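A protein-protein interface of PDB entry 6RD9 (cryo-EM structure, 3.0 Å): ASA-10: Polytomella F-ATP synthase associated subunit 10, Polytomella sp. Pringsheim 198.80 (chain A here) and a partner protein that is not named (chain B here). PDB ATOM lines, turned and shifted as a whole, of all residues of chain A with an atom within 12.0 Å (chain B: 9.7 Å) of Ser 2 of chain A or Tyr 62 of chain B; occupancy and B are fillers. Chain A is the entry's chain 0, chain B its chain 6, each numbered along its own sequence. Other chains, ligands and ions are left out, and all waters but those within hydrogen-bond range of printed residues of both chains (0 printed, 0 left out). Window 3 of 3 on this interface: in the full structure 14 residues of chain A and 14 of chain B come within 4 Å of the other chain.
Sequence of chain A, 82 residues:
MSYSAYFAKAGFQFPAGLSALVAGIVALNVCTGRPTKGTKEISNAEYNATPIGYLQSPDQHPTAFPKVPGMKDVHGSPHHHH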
ATOM      1  N   SER A   2       0.124   3.182 -23.371  1.00  0.00           N
ATOM      2  CA  SER A   2       0.854   2.297 -22.498  1.00  0.00           C
ATOM      3  C   SER A   2       2.246   2.204 -23.028  1.00  0.00           C
ATOM      4  O   SER A   2       2.513   1.395 -23.892  1.00  0.00           O
ATOM      5  CB  SER A   2       0.188   0.930 -22.430  1.00  0.00           C
ATOM      6  OG  SER A   2      -0.968   0.972 -21.614  1.00  0.00           O
ATOM      7  N   TYR A   3       3.092   3.127 -22.571  1.00  0.00           N
ATOM      8  CA  TYR A   3       4.526   3.248 -22.834  1.00  0.00           C
ATOM      9  C   TYR A   3       4.871   3.591 -24.271  1.00  0.00           C
ATOM     10  O   TYR A   3       6.036   3.829 -24.558  1.00  0.00           O
ATOM     11  CB  TYR A   3       5.295   1.984 -22.455  1.00  0.00           C
ATOM     12  CG  TYR A   3       5.442   1.753 -20.992  1.00  0.00           C
ATOM     13  CD1 TYR A   3       5.686   2.789 -20.143  1.00  0.00           C
ATOM     14  CD2 TYR A   3       5.332   0.488 -20.467  1.00  0.00           C
ATOM     15  CE1 TYR A   3       5.793   2.576 -18.819  1.00  0.00           C
ATOM     16  CE2 TYR A   3       5.450   0.276 -19.148  1.00  0.00           C
ATOM     17  CZ  TYR A   3       5.676   1.326 -18.331  1.00  0.00           C
ATOM     18  OH  TYR A   3       5.791   1.150 -16.988  1.00  0.00           O
ATOM     19  N   SER A   4       3.906   3.639 -25.185  1.00  0.00           N
ATOM     20  CA  SER A   4       4.221   4.038 -26.547  1.00  0.00           C
ATOM     21  C   SER A   4       4.503   5.518 -26.633  1.00  0.00           C
ATOM     22  O   SER A   4       5.319   5.945 -27.443  1.00  0.00           O
ATOM     23  CB  SER A   4       3.082   3.695 -27.493  1.00  0.00           C
ATOM     24  OG  SER A   4       2.991   2.311 -27.712  1.00  0.00           O
ATOM     25  N   ALA A   5       3.846   6.307 -25.809  1.00  0.00           N
ATOM     26  CA  ALA A   5       4.031   7.741 -25.791  1.00  0.00           C
ATOM     27  C   ALA A   5       5.212   8.179 -24.955  1.00  0.00           C
ATOM     28  O   ALA A   5       5.521   9.367 -24.932  1.00  0.00           O
ATOM     29  CB  ALA A   5       2.772   8.395 -25.261  1.00  0.00           C
ATOM     30  N   TYR A   6       5.846   7.269 -24.236  1.00  0.00           N
ATOM     31  CA  TYR A   6       7.071   7.604 -23.534  1.00  0.00           C
ATOM     32  C   TYR A   6       8.262   7.542 -24.466  1.00  0.00           C
ATOM     33  O   TYR A   6       9.230   8.284 -24.292  1.00  0.00           O
ATOM     34  CB  TYR A   6       7.256   6.654 -22.360  1.00  0.00           C
ATOM     35  CG  TYR A   6       8.595   6.712 -21.718  1.00  0.00           C
ATOM     36  CD1 TYR A   6       9.004   7.831 -21.051  1.00  0.00           C
ATOM     37  CD2 TYR A   6       9.451   5.650 -21.788  1.00  0.00           C
ATOM     38  CE1 TYR A   6      10.233   7.887 -20.472  1.00  0.00           C
ATOM     39  CE2 TYR A   6      10.671   5.695 -21.212  1.00  0.00           C
ATOM     40  CZ  TYR A   6      11.061   6.813 -20.556  1.00  0.00           C
ATOM     41  OH  TYR A   6      12.296   6.868 -19.975  1.00  0.00           O
ATOM     42  N   PHE A   7       8.198   6.677 -25.461  1.00  0.00           N
ATOM     43  CA  PHE A   7       9.270   6.510 -26.416  1.00  0.00           C
ATOM     44  C   PHE A   7       9.160   7.442 -27.597  1.00  0.00           C
ATOM     45  O   PHE A   7      10.116   7.549 -28.366  1.00  0.00           O
ATOM     46  CB  PHE A   7       9.304   5.075 -26.895  1.00  0.00           C
ATOM     47  CG  PHE A   7       9.719   4.136 -25.850  1.00  0.00           C
ATOM     48  CD1 PHE A   7      10.898   4.336 -25.175  1.00  0.00           C
ATOM     49  CD2 PHE A   7       8.933   3.081 -25.515  1.00  0.00           C
ATOM     50  CE1 PHE A   7      11.270   3.492 -24.203  1.00  0.00           C
ATOM     51  CE2 PHE A   7       9.309   2.241 -24.541  1.00  0.00           C
ATOM     52  CZ  PHE A   7      10.474   2.449 -23.889  1.00  0.00           C
ATOM     53  N   ALA A   8       8.035   8.113 -27.762  1.00  0.00           N
ATOM     54  CA  ALA A   8       7.955   9.154 -28.764  1.00  0.00           C
ATOM     55  C   ALA A   8       8.485  10.482 -28.262  1.00  0.00           C
ATOM     56  O   ALA A   8       8.714  11.379 -29.072  1.00  0.00           O
ATOM     57  CB  ALA A   8       6.514   9.307 -29.229  1.00  0.00           C
ATOM     58  N   LYS A   9       8.692  10.624 -26.957  1.00  0.00           N
ATOM     59  CA  LYS A   9       9.114  11.897 -26.387  1.00  0.00           C
ATOM     60  C   LYS A   9      10.568  12.194 -26.692  1.00  0.00           C
ATOM     61  O   LYS A   9      10.900  13.280 -27.170  1.00  0.00           O
ATOM     62  CB  LYS A   9       8.889  11.904 -24.883  1.00  0.00           C
ATOM     63  CG  LYS A   9       7.449  12.004 -24.513  1.00  0.00           C
ATOM     64  CD  LYS A   9       7.274  11.878 -23.031  1.00  0.00           C
ATOM     65  CE  LYS A   9       5.815  11.841 -22.683  1.00  0.00           C
ATOM     66  NZ  LYS A   9       5.628  12.105 -21.246  1.00  0.00           N
ATOM     67  N   ALA B  56      -6.998   2.661  -9.522  1.00  0.00           N
ATOM     68  CA  ALA B  56      -6.352   3.655 -10.356  1.00  0.00           C
ATOM     69  C   ALA B  56      -5.280   4.437  -9.627  1.00  0.00           C
ATOM     70  O   ALA B  56      -4.483   5.105 -10.276  1.00  0.00           O
ATOM     71  CB  ALA B  56      -7.392   4.614 -10.908  1.00  0.00           C
ATOM     72  N   ALA B  58      -3.059   2.864  -7.955  1.00  0.00           N
ATOM     73  CA  ALA B  58      -1.958   1.921  -7.998  1.00  0.00           C
ATOM     74  C   ALA B  58      -1.719   1.382  -9.391  1.00  0.00           C
ATOM     75  O   ALA B  58      -0.969   0.421  -9.547  1.00  0.00           O
ATOM     76  CB  ALA B  58      -2.219   0.763  -7.053  1.00  0.00           C
ATOM     77  N   ALA B  59      -2.365   1.950 -10.393  1.00  0.00           N
ATOM     78  CA  ALA B  59      -2.024   1.654 -11.760  1.00  0.00           C
ATOM     79  C   ALA B  59      -0.665   2.262 -12.069  1.00  0.00           C
ATOM     80  O   ALA B  59      -0.293   3.272 -11.477  1.00  0.00           O
ATOM     81  CB  ALA B  59      -3.079   2.219 -12.693  1.00  0.00           C
ATOM     82  N   PRO B  60       0.112   1.656 -12.960  1.00  0.00           N
ATOM     83  CA  PRO B  60       1.402   2.241 -13.309  1.00  0.00           C
ATOM     84  C   PRO B  60       1.226   3.454 -14.197  1.00  0.00           C
ATOM     85  O   PRO B  60       0.221   3.615 -14.884  1.00  0.00           O
ATOM     86  CB  PRO B  60       2.105   1.112 -14.044  1.00  0.00           C
ATOM     87  CG  PRO B  60       1.040   0.333 -14.587  1.00  0.00           C
ATOM     88  CD  PRO B  60      -0.057   0.351 -13.611  1.00  0.00           C
ATOM     89  N   ILE B  61       2.221   4.328 -14.171  1.00  0.00           N
ATOM     90  CA  ILE B  61       2.168   5.519 -15.003  1.00  0.00           C
ATOM     91  C   ILE B  61       2.512   5.130 -16.429  1.00  0.00           C
ATOM     92  O   ILE B  61       3.488   4.424 -16.683  1.00  0.00           O
ATOM     93  CB  ILE B  61       3.084   6.629 -14.458  1.00  0.00           C
ATOM     94  CG1 ILE B  61       3.021   7.860 -15.339  1.00  0.00           C
ATOM     95  CG2 ILE B  61       4.522   6.203 -14.307  1.00  0.00           C
ATOM     96  CD1 ILE B  61       1.719   8.548 -15.279  1.00  0.00           C
ATOM     97  N   TYR B  62       1.647   5.488 -17.348  1.00  0.00           N
ATOM     98  CA  TYR B  62       1.965   5.435 -18.762  1.00  0.00           C
ATOM     99  C   TYR B  62       1.899   6.868 -19.222  1.00  0.00           C
ATOM    100  O   TYR B  62       0.786   7.411 -19.339  1.00  0.00           O
ATOM    101  CB  TYR B  62       0.968   4.578 -19.521  1.00  0.00           C
ATOM    102  CG  TYR B  62       0.872   3.173 -19.024  1.00  0.00           C
ATOM    103  CD1 TYR B  62       1.993   2.446 -18.736  1.00  0.00           C
ATOM    104  CD2 TYR B  62      -0.351   2.571 -18.848  1.00  0.00           C
ATOM    105  CE1 TYR B  62       1.902   1.170 -18.292  1.00  0.00           C
ATOM    106  CE2 TYR B  62      -0.442   1.296 -18.402  1.00  0.00           C
ATOM    107  CZ  TYR B  62       0.691   0.603 -18.129  1.00  0.00           C
ATOM    108  OH  TYR B  62       0.598  -0.679 -17.685  1.00  0.00           O
ATOM    109  N   PRO B  63       3.036   7.520 -19.460  1.00  0.00           N
ATOM    110  CA  PRO B  63       3.043   8.964 -19.672  1.00  0.00           C
ATOM    111  C   PRO B  63       2.305   9.375 -20.927  1.00  0.00           C
ATOM    112  O   PRO B  63       2.251   8.637 -21.909  1.00  0.00           O
ATOM    113  CB  PRO B  63       4.532   9.282 -19.768  1.00  0.00           C
ATOM    114  CG  PRO B  63       5.159   8.235 -19.005  1.00  0.00           C
ATOM    115  CD  PRO B  63       4.395   7.013 -19.289  1.00  0.00           C
ATOM    116  N   ALA B  64       1.656  10.525 -20.847  1.00  0.00           N
ATOM    117  CA  ALA B  64       0.718  10.914 -21.875  1.00  0.00           C
ATOM    118  C   ALA B  64       1.447  11.513 -23.061  1.00  0.00           C
ATOM    119  O   ALA B  64       2.541  12.065 -22.937  1.00  0.00           O
ATOM    120  CB  ALA B  64      -0.300  11.903 -21.322  1.00  0.00           C
ATOM    121  N   ALA B  65       0.809  11.414 -24.219  1.00  0.00           N
ATOM    122  CA  ALA B  65       1.402  11.812 -25.487  1.00  0.00           C
ATOM    123  C   ALA B  65       1.533  13.320 -25.529  1.00  0.00           C
ATOM    124  O   ALA B  65       0.554  14.030 -25.748  1.00  0.00           O
ATOM    125  CB  ALA B  65       0.551  11.301 -26.641  1.00  0.00           C
ATOM    126  N   ALA B  66       2.747  13.817 -25.327  1.00  0.00           N
ATOM    127  CA  ALA B  66       2.969  15.253 -25.304  1.00  0.00           C
ATOM    128  C   ALA B  66       2.870  15.843 -26.708  1.00  0.00           C
ATOM    129  O   ALA B  66       2.691  15.134 -27.702  1.00  0.00           O
ATOM    130  CB  ALA B  66       4.330  15.576 -24.692  1.00  0.00           C
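Among the printed residues, pairs that only touch across the chains: Ser 2 of chain A with Tyr 62 of chain B (3.3 Å), Lys 9 of chain A with Ala 64 of chain B (3.3 Å), Lys 9 of chain A with Pro 63 of chain B (3.4 Å), Ala 5 of chain A with Pro 63 of chain B (3.4 Å), Tyr 3 of chain A with Ile 61 of chain B (3.6 Å), Ala 5 of chain A with Ala 65 of chain B (3.7 Å) and Tyr 3 of chain A with Tyr 62 of chain B (3.8 Å).
Ser 2 of chain A touches just one residue of chain B: Tyr 62 (3.3 Å). Tyr 62 of chain B touches just these residues of chain A: Ser 2 and Tyr 3. Of chain B, only Ile 61 (3.6 Å) and Tyr 62 (3.8 Å) come within 4 Å of Tyr 3 of chain A. No residue of chain A comes within 4 Å of Pro 60 of chain B. Of chain A, only Tyr 3 comes within 4 Å of Ile 61 of chain B. Ala 64 of chain B touches just one residue of chain A: Lys 9 (3.3 Å). Of the printed residues of chain B, Lys 9 of chain A touches Pro 63 and Ala 64. Of the printed residues of chain A, Ala 65 of chain B touches Ala 5 (3.7 Å). Of the printed residues of chain B, Ala 5 of chain A touches Pro 63 and Ala 65. Ala 56 of chain B touches none of the printed residues of chain A.
Of the 10 printed residues of chain B, 5 touch a printed residue of chain A. Printed residues of chain B that touch a printed residue of chain A: Ile 61, Tyr 62, Pro 63, Ala 64 and Ala 65. Of the 8 printed residues of chain A, 4 touch a printed residue of chain B. Printed residues of chain A that touch a printed residue of chain B: Ser 2, Tyr 3, Ala 5 and Lys 9. Among the printed residues, 7 pairs touch across the chains.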
